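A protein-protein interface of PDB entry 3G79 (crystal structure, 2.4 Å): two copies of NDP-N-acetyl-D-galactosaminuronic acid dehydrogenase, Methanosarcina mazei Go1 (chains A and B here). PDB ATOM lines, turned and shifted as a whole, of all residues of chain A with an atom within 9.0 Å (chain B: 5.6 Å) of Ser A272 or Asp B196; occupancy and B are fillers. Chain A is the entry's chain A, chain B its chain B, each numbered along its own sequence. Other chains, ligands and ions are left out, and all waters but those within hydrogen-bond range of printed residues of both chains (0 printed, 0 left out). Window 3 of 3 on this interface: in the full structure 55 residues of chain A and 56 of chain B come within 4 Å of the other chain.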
ATOM      1  N   ASP A 265     -17.563 -32.184 -12.010  1.00  0.00           N
ATOM      2  CA  ASP A 265     -17.185 -32.598 -10.677  1.00  0.00           C
ATOM      3  C   ASP A 265     -15.707 -32.285 -10.501  1.00  0.00           C
ATOM      4  O   ASP A 265     -15.273 -31.855  -9.427  1.00  0.00           O
ATOM      5  CB  ASP A 265     -17.409 -34.098 -10.499  1.00  0.00           C
ATOM      6  CG  ASP A 265     -18.888 -34.486 -10.401  1.00  0.00           C
ATOM      7  OD1 ASP A 265     -19.754 -33.703  -9.905  1.00  0.00           O
ATOM      8  OD2 ASP A 265     -19.169 -35.629 -10.813  1.00  0.00           O
ATOM      9  N   VAL A 266     -14.937 -32.481 -11.565  1.00  0.00           N
ATOM     10  CA  VAL A 266     -13.510 -32.182 -11.498  1.00  0.00           C
ATOM     11  C   VAL A 266     -13.432 -30.712 -11.227  1.00  0.00           C
ATOM     12  O   VAL A 266     -12.905 -30.301 -10.189  1.00  0.00           O
ATOM     13  CB  VAL A 266     -12.715 -32.710 -12.738  1.00  0.00           C
ATOM     14  CG1 VAL A 266     -11.210 -32.404 -12.656  1.00  0.00           C
ATOM     15  CG2 VAL A 266     -12.908 -34.254 -12.841  1.00  0.00           C
ATOM     16  N   ARG A 267     -14.091 -29.944 -12.077  1.00  0.00           N
ATOM     17  CA  ARG A 267     -14.129 -28.490 -11.972  1.00  0.00           C
ATOM     18  C   ARG A 267     -14.620 -27.926 -10.608  1.00  0.00           C
ATOM     19  O   ARG A 267     -13.960 -27.047 -10.018  1.00  0.00           O
ATOM     20  CB  ARG A 267     -14.958 -27.902 -13.102  1.00  0.00           C
ATOM     21  CG  ARG A 267     -15.134 -26.430 -12.910  1.00  0.00           C
ATOM     22  CD  ARG A 267     -15.885 -25.782 -14.026  1.00  0.00           C
ATOM     23  NE  ARG A 267     -15.822 -24.370 -13.751  1.00  0.00           N
ATOM     24  CZ  ARG A 267     -16.544 -23.758 -12.823  1.00  0.00           C
ATOM     25  NH1 ARG A 267     -17.439 -24.429 -12.135  1.00  0.00           N
ATOM     26  NH2 ARG A 267     -16.383 -22.460 -12.613  1.00  0.00           N
ATOM     27  N   THR A 268     -15.746 -28.404 -10.084  1.00  0.00           N
ATOM     28  CA  THR A 268     -16.119 -27.970  -8.720  1.00  0.00           C
ATOM     29  C   THR A 268     -15.067 -28.367  -7.660  1.00  0.00           C
ATOM     30  O   THR A 268     -14.686 -27.541  -6.819  1.00  0.00           O
ATOM     31  CB  THR A 268     -17.638 -28.157  -8.297  1.00  0.00           C
ATOM     32  OG1 THR A 268     -17.751 -28.749  -6.990  1.00  0.00           O
ATOM     33  CG2 THR A 268     -18.433 -28.935  -9.270  1.00  0.00           C
ATOM     34  N   GLY A 269     -14.549 -29.585  -7.744  1.00  0.00           N
ATOM     35  CA  GLY A 269     -13.387 -29.961  -6.947  1.00  0.00           C
ATOM     36  C   GLY A 269     -12.271 -28.936  -7.027  1.00  0.00           C
ATOM     37  O   GLY A 269     -11.912 -28.353  -6.001  1.00  0.00           O
ATOM     38  N   VAL A 270     -11.750 -28.673  -8.237  1.00  0.00           N
ATOM     39  CA  VAL A 270     -10.664 -27.704  -8.414  1.00  0.00           C
ATOM     40  C   VAL A 270     -10.997 -26.322  -7.816  1.00  0.00           C
ATOM     41  O   VAL A 270     -10.189 -25.693  -7.119  1.00  0.00           O
ATOM     42  CB  VAL A 270     -10.337 -27.471  -9.909  1.00  0.00           C
ATOM     43  CG1 VAL A 270      -9.467 -26.263 -10.073  1.00  0.00           C
ATOM     44  CG2 VAL A 270      -9.638 -28.642 -10.531  1.00  0.00           C
ATOM     45  N   ASP A 271     -12.199 -25.855  -8.120  1.00  0.00           N
ATOM     46  CA  ASP A 271     -12.667 -24.537  -7.778  1.00  0.00           C
ATOM     47  C   ASP A 271     -12.840 -24.356  -6.278  1.00  0.00           C
ATOM     48  O   ASP A 271     -13.092 -23.247  -5.812  1.00  0.00           O
ATOM     49  CB  ASP A 271     -13.969 -24.300  -8.537  1.00  0.00           C
ATOM     50  CG  ASP A 271     -14.579 -22.966  -8.251  1.00  0.00           C
ATOM     51  OD1 ASP A 271     -14.057 -21.974  -8.791  1.00  0.00           O
ATOM     52  OD2 ASP A 271     -15.587 -22.918  -7.502  1.00  0.00           O
ATOM     53  N   SER A 272     -12.674 -25.424  -5.512  1.00  0.00           N
ATOM     54  CA  SER A 272     -12.787 -25.313  -4.056  1.00  0.00           C
ATOM     55  C   SER A 272     -11.517 -24.785  -3.421  1.00  0.00           C
ATOM     56  O   SER A 272     -11.408 -24.746  -2.189  1.00  0.00           O
ATOM     57  CB  SER A 272     -13.111 -26.651  -3.414  1.00  0.00           C
ATOM     58  OG  SER A 272     -11.926 -27.347  -3.101  1.00  0.00           O
ATOM     59  N   LEU A 273     -10.538 -24.432  -4.246  1.00  0.00           N
ATOM     60  CA  LEU A 273      -9.347 -23.739  -3.766  1.00  0.00           C
ATOM     61  C   LEU A 273      -9.529 -22.230  -3.937  1.00  0.00           C
ATOM     62  O   LEU A 273      -9.628 -21.717  -5.071  1.00  0.00           O
ATOM     63  CB  LEU A 273      -8.122 -24.233  -4.514  1.00  0.00           C
ATOM     64  CG  LEU A 273      -7.718 -25.615  -4.028  1.00  0.00           C
ATOM     65  CD1 LEU A 273      -7.227 -26.485  -5.178  1.00  0.00           C
ATOM     66  CD2 LEU A 273      -6.654 -25.423  -2.958  1.00  0.00           C
ATOM     67  N   LYS A 274      -9.583 -21.531  -2.807  1.00  0.00           N
ATOM     68  CA  LYS A 274     -10.018 -20.131  -2.800  1.00  0.00           C
ATOM     69  C   LYS A 274      -8.855 -19.157  -2.628  1.00  0.00           C
ATOM     70  O   LYS A 274      -7.964 -19.388  -1.797  1.00  0.00           O
ATOM     71  CB  LYS A 274     -11.101 -19.887  -1.733  1.00  0.00           C
ATOM     72  CG  LYS A 274     -12.558 -19.931  -2.210  1.00  0.00           C
ATOM     73  CD  LYS A 274     -12.973 -21.235  -2.863  1.00  0.00           C
ATOM     74  CE  LYS A 274     -14.390 -21.096  -3.391  1.00  0.00           C
ATOM     75  NZ  LYS A 274     -14.594 -21.569  -4.791  1.00  0.00           N
ATOM     76  N   GLY A 275      -8.897 -18.075  -3.428  1.00  0.00           N
ATOM     77  CA  GLY A 275      -7.776 -17.118  -3.589  1.00  0.00           C
ATOM     78  C   GLY A 275      -7.608 -16.168  -2.424  1.00  0.00           C
ATOM     79  O   GLY A 275      -8.292 -16.327  -1.380  1.00  0.00           O
ATOM     80  N   ILE A 278      -4.173 -17.919  -5.020  1.00  0.00           N
ATOM     81  CA  ILE A 278      -4.423 -19.363  -4.882  1.00  0.00           C
ATOM     82  C   ILE A 278      -5.443 -19.884  -5.930  1.00  0.00           C
ATOM     83  O   ILE A 278      -5.150 -20.869  -6.630  1.00  0.00           O
ATOM     84  CB  ILE A 278      -4.801 -19.738  -3.410  1.00  0.00           C
ATOM     85  CG1 ILE A 278      -3.652 -20.469  -2.684  1.00  0.00           C
ATOM     86  CG2 ILE A 278      -5.960 -20.694  -3.379  1.00  0.00           C
ATOM     87  CD1 ILE A 278      -2.484 -19.635  -2.202  1.00  0.00           C
ATOM     88  N   THR A 279      -6.605 -19.225  -6.055  1.00  0.00           N
ATOM     89  CA  THR A 279      -7.635 -19.637  -7.031  1.00  0.00           C
ATOM     90  C   THR A 279      -7.025 -20.048  -8.358  1.00  0.00           C
ATOM     91  O   THR A 279      -6.089 -19.412  -8.848  1.00  0.00           O
ATOM     92  CB  THR A 279      -8.687 -18.512  -7.461  1.00  0.00           C
ATOM     93  OG1 THR A 279      -8.531 -17.293  -6.711  1.00  0.00           O
ATOM     94  CG2 THR A 279     -10.124 -19.040  -7.415  1.00  0.00           C
ATOM     95  N   ARG A 280      -7.582 -21.092  -8.948  1.00  0.00           N
ATOM     96  CA  ARG A 280      -7.256 -21.458 -10.308  1.00  0.00           C
ATOM     97  C   ARG A 280      -8.215 -20.764 -11.253  1.00  0.00           C
ATOM     98  O   ARG A 280      -8.063 -20.839 -12.459  1.00  0.00           O
ATOM     99  CB  ARG A 280      -7.308 -22.973 -10.476  1.00  0.00           C
ATOM    100  CG  ARG A 280      -5.948 -23.615 -10.278  1.00  0.00           C
ATOM    101  CD  ARG A 280      -5.842 -24.535  -9.070  1.00  0.00           C
ATOM    102  NE  ARG A 280      -5.368 -23.828  -7.912  1.00  0.00           N
ATOM    103  CZ  ARG A 280      -4.391 -24.230  -7.088  1.00  0.00           C
ATOM    104  NH1 ARG A 280      -3.753 -25.357  -7.286  1.00  0.00           N
ATOM    105  NH2 ARG A 280      -4.052 -23.459  -6.056  1.00  0.00           N
ATOM    106  N   ALA A 281      -9.200 -20.073 -10.674  1.00  0.00           N
ATOM    107  CA  ALA A 281     -10.182 -19.262 -11.411  1.00  0.00           C
ATOM    108  C   ALA A 281     -10.727 -19.955 -12.663  1.00  0.00           C
ATOM    109  O   ALA A 281     -10.719 -19.395 -13.739  1.00  0.00           O
ATOM    110  CB  ALA A 281      -9.597 -17.900 -11.744  1.00  0.00           C
ATOM    111  N   VAL A 282     -11.223 -21.167 -12.466  1.00  0.00           N
ATOM    112  CA  VAL A 282     -11.652 -22.091 -13.531  1.00  0.00           C
ATOM    113  C   VAL A 282     -12.971 -21.693 -14.206  1.00  0.00           C
ATOM    114  O   VAL A 282     -14.040 -21.643 -13.569  1.00  0.00           O
ATOM    115  CB  VAL A 282     -11.817 -23.532 -12.989  1.00  0.00           C
ATOM    116  CG1 VAL A 282     -12.053 -24.518 -14.112  1.00  0.00           C
ATOM    117  CG2 VAL A 282     -10.607 -23.947 -12.237  1.00  0.00           C
ATOM    118  N   ARG B 182      -5.620 -32.964   0.660  1.00  0.00           N
ATOM    119  CA  ARG B 182      -4.859 -31.745   0.398  1.00  0.00           C
ATOM    120  C   ARG B 182      -4.477 -31.112   1.728  1.00  0.00           C
ATOM    121  O   ARG B 182      -5.337 -30.547   2.404  1.00  0.00           O
ATOM    122  CB  ARG B 182      -5.700 -30.748  -0.399  1.00  0.00           C
ATOM    123  CG  ARG B 182      -5.612 -30.882  -1.917  1.00  0.00           C
ATOM    124  CD  ARG B 182      -6.853 -31.583  -2.492  1.00  0.00           C
ATOM    125  NE  ARG B 182      -7.593 -30.782  -3.487  1.00  0.00           N
ATOM    126  CZ  ARG B 182      -8.116 -29.560  -3.287  1.00  0.00           C
ATOM    127  NH1 ARG B 182      -7.970 -28.918  -2.127  1.00  0.00           N
ATOM    128  NH2 ARG B 182      -8.782 -28.964  -4.273  1.00  0.00           N
ATOM    129  N   GLU B 194     -11.178 -27.401   7.993  1.00  0.00           N
ATOM    130  CA  GLU B 194     -11.676 -26.146   7.464  1.00  0.00           C
ATOM    131  C   GLU B 194     -11.846 -26.073   5.951  1.00  0.00           C
ATOM    132  O   GLU B 194     -12.600 -25.243   5.450  1.00  0.00           O
ATOM    133  CB  GLU B 194     -10.906 -24.955   8.056  1.00  0.00           C
ATOM    134  CG  GLU B 194     -11.234 -24.793   9.573  1.00  0.00           C
ATOM    135  CD  GLU B 194     -11.055 -23.384  10.107  1.00  0.00           C
ATOM    136  OE1 GLU B 194     -10.657 -22.522   9.287  1.00  0.00           O
ATOM    137  OE2 GLU B 194     -11.285 -23.149  11.333  1.00  0.00           O
ATOM    138  N   HIS B 195     -11.196 -26.947   5.205  1.00  0.00           N
ATOM    139  CA  HIS B 195     -11.531 -26.917   3.799  1.00  0.00           C
ATOM    140  C   HIS B 195     -12.263 -28.128   3.237  1.00  0.00           C
ATOM    141  O   HIS B 195     -12.430 -29.139   3.917  1.00  0.00           O
ATOM    142  CB  HIS B 195     -10.440 -26.305   2.883  1.00  0.00           C
ATOM    143  CG  HIS B 195      -9.037 -26.767   3.143  1.00  0.00           C
ATOM    144  ND1 HIS B 195      -7.978 -25.883   3.232  1.00  0.00           N
ATOM    145  CD2 HIS B 195      -8.501 -28.006   3.230  1.00  0.00           C
ATOM    146  CE1 HIS B 195      -6.855 -26.560   3.398  1.00  0.00           C
ATOM    147  NE2 HIS B 195      -7.145 -27.851   3.414  1.00  0.00           N
ATOM    148  N   ASP B 196     -12.782 -27.975   2.027  1.00  0.00           N
ATOM    149  CA  ASP B 196     -13.635 -28.975   1.463  1.00  0.00           C
ATOM    150  C   ASP B 196     -12.813 -30.224   1.218  1.00  0.00           C
ATOM    151  O   ASP B 196     -11.653 -30.120   0.836  1.00  0.00           O
ATOM    152  CB  ASP B 196     -14.295 -28.449   0.187  1.00  0.00           C
ATOM    153  CG  ASP B 196     -15.226 -27.273   0.458  1.00  0.00           C
ATOM    154  OD1 ASP B 196     -15.651 -26.579  -0.491  1.00  0.00           O
ATOM    155  OD2 ASP B 196     -15.542 -27.046   1.648  1.00  0.00           O
ATOM    156  N   ARG B 197     -13.411 -31.385   1.477  1.00  0.00           N
ATOM    157  CA  ARG B 197     -12.835 -32.702   1.170  1.00  0.00           C
ATOM    158  C   ARG B 197     -13.506 -33.332  -0.082  1.00  0.00           C
ATOM    159  O   ARG B 197     -14.739 -33.506  -0.120  1.00  0.00           O
ATOM    160  CB  ARG B 197     -13.030 -33.632   2.373  1.00  0.00           C
ATOM    161  CG  ARG B 197     -12.138 -34.885   2.448  1.00  0.00           C
ATOM    162  CD  ARG B 197     -10.703 -34.503   2.475  1.00  0.00           C
ATOM    163  NE  ARG B 197      -9.880 -35.698   2.378  1.00  0.00           N
ATOM    164  CZ  ARG B 197      -9.509 -36.411   3.440  1.00  0.00           C
ATOM    165  NH1 ARG B 197      -9.866 -36.042   4.651  1.00  0.00           N
ATOM    166  NH2 ARG B 197      -8.790 -37.475   3.290  1.00  0.00           N
ATOM    167  N   ILE B 198     -12.687 -33.651  -1.091  1.00  0.00           N
ATOM    168  CA  ILE B 198     -13.110 -34.431  -2.260  1.00  0.00           C
ATOM    169  C   ILE B 198     -13.180 -35.930  -1.922  1.00  0.00           C
ATOM    170  O   ILE B 198     -12.192 -36.524  -1.401  1.00  0.00           O
ATOM    171  CB  ILE B 198     -12.065 -34.374  -3.405  1.00  0.00           C
ATOM    172  CG1 ILE B 198     -11.621 -32.935  -3.729  1.00  0.00           C
ATOM    173  CG2 ILE B 198     -12.562 -35.177  -4.639  1.00  0.00           C
ATOM    174  CD1 ILE B 198     -12.708 -32.056  -4.105  1.00  0.00           C
ATOM    175  N   LEU B 218     -15.584 -32.505   9.865  1.00  0.00           N
ATOM    176  CA  LEU B 218     -15.526 -31.155   9.286  1.00  0.00           C
ATOM    177  C   LEU B 218     -16.219 -30.057  10.076  1.00  0.00           C
ATOM    178  O   LEU B 218     -17.365 -30.195  10.455  1.00  0.00           O
ATOM    179  CB  LEU B 218     -16.060 -31.140   7.840  1.00  0.00           C
ATOM    180  CG  LEU B 218     -15.346 -32.001   6.798  1.00  0.00           C
ATOM    181  CD1 LEU B 218     -15.952 -31.751   5.427  1.00  0.00           C
ATOM    182  CD2 LEU B 218     -13.902 -31.696   6.757  1.00  0.00           C
ATOM    183  N   VAL B 220     -16.643 -26.476   8.859  1.00  0.00           N
ATOM    184  CA  VAL B 220     -16.501 -25.368   7.865  1.00  0.00           C
ATOM    185  C   VAL B 220     -16.235 -25.934   6.498  1.00  0.00           C
ATOM    186  O   VAL B 220     -16.666 -25.364   5.507  1.00  0.00           O
ATOM    187  CB  VAL B 220     -15.444 -24.205   8.201  1.00  0.00           C
ATOM    188  CG1 VAL B 220     -15.338 -23.204   7.040  1.00  0.00           C
ATOM    189  CG2 VAL B 220     -15.869 -23.397   9.394  1.00  0.00           C
ATOM    190  N   GLY B 221     -15.512 -27.043   6.443  1.00  0.00           N
ATOM    191  CA  GLY B 221     -15.357 -27.768   5.187  1.00  0.00           C
ATOM    192  C   GLY B 221     -16.609 -28.562   4.874  1.00  0.00           C
ATOM    193  O   GLY B 221     -17.343 -28.921   5.768  1.00  0.00           O
ATOM    194  N   GLN B 222     -16.861 -28.809   3.593  1.00  0.00           N
ATOM    195  CA  GLN B 222     -17.957 -29.660   3.166  1.00  0.00           C
ATOM    196  C   GLN B 222     -17.286 -30.768   2.438  1.00  0.00           C
ATOM    197  O   GLN B 222     -16.146 -30.618   2.048  1.00  0.00           O
ATOM    198  CB  GLN B 222     -18.837 -28.926   2.176  1.00  0.00           C
ATOM    199  CG  GLN B 222     -19.435 -27.670   2.741  1.00  0.00           C
ATOM    200  CD  GLN B 222     -20.787 -27.405   2.164  1.00  0.00           C
ATOM    201  OE1 GLN B 222     -20.901 -26.935   1.028  1.00  0.00           O
ATOM    202  NE2 GLN B 222     -21.840 -27.738   2.924  1.00  0.00           N
ATOM    203  N   VAL B 223     -17.996 -31.867   2.226  1.00  0.00           N
ATOM    204  CA  VAL B 223     -17.510 -32.926   1.410  1.00  0.00           C
ATOM    205  C   VAL B 223     -17.975 -32.626  -0.017  1.00  0.00           C
ATOM    206  O   VAL B 223     -19.115 -32.236  -0.226  1.00  0.00           O
ATOM    207  CB  VAL B 223     -18.026 -34.280   1.893  1.00  0.00           C
ATOM    208  CG1 VAL B 223     -17.747 -35.369   0.866  1.00  0.00           C
ATOM    209  CG2 VAL B 223     -17.399 -34.628   3.286  1.00  0.00           C
ATOM    210  N   ILE B 224     -17.064 -32.791  -0.986  1.00  0.00           N
ATOM    211  CA  ILE B 224     -17.387 -32.693  -2.406  1.00  0.00           C
ATOM    212  C   ILE B 224     -17.466 -34.082  -3.025  1.00  0.00           C
ATOM    213  O   ILE B 224     -16.453 -34.664  -3.388  1.00  0.00           O
ATOM    214  CB  ILE B 224     -16.417 -31.752  -3.153  1.00  0.00           C
ATOM    215  CG1 ILE B 224     -16.384 -30.383  -2.431  1.00  0.00           C
ATOM    216  CG2 ILE B 224     -16.883 -31.602  -4.609  1.00  0.00           C
ATOM    217  CD1 ILE B 224     -15.652 -29.207  -3.136  1.00  0.00           C
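The side-chain hydroxyl of Ser A272 sits at hydrogen-bond distance from the backbone carbonyl oxygen of Gly A269 (3.1 Å).
A ring nitrogen (NE2) of His B195 is in hydrogen-bond range of the backbone carbonyl oxygen (O) of Arg B182 (3.4 Å).
The backbone NH of Gln B222 lies within hydrogen-bond range of the side-chain carboxylate of Asp B196, 2.9 Å away.
The backbone NH of Ile B224 is in hydrogen-bond range of the backbone carbonyl oxygen of Arg B197, at 2.6 Å.
Among the printed residues, pairs that only touch across the chains: Thr A268 with Ile B224 (3.8 Å), Gly A269 with Arg B182 (3.6 Å), Gly A269 with Ile B198 (3.6 Å), Ser A272 with Arg B182 (3.7 Å), Ser A272 with Asp B196 (3.9 Å), Ser A272 with Ile B224 (3.6 Å) and Leu A273 with Arg B182 (3.1 Å).
Of chain B, only Arg B182 (3.7 Å), Asp B196 (3.9 Å) and Ile B224 (3.6 Å) come within 4 Å of Ser A272.
Of chain A, only Ser A272 (3.9 Å) comes within 4 Å of Asp B196.
No residue of chain A comes within 4 Å of Gly B221.
Of the printed residues of chain B, Thr A268 touches Ile B224.
Of the printed residues of chain A, Arg B182 touches Gly A269 (3.6 Å), Ser A272 (3.7 Å) and Leu A273 (3.1 Å).
Arg A280 touches none of the printed residues of chain B.
Arg A267 touches none of the printed residues of chain B.
The nearest residue of chain A that does not touch Asp B196 is Lys A274 (6.3 Å).
The nearest printed residue of chain B that does not touch Gly A269 is Ile B224 (4.4 Å).
Of the 12 printed residues of chain B, 4 touch a printed residue of chain A.
Among the printed residues, 7 pairs touch across the chains.
No position is printed for both chains.
Of the 7 pairs that touch across the chains among the printed residues, none has its exchanged pair printed and touching as well.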
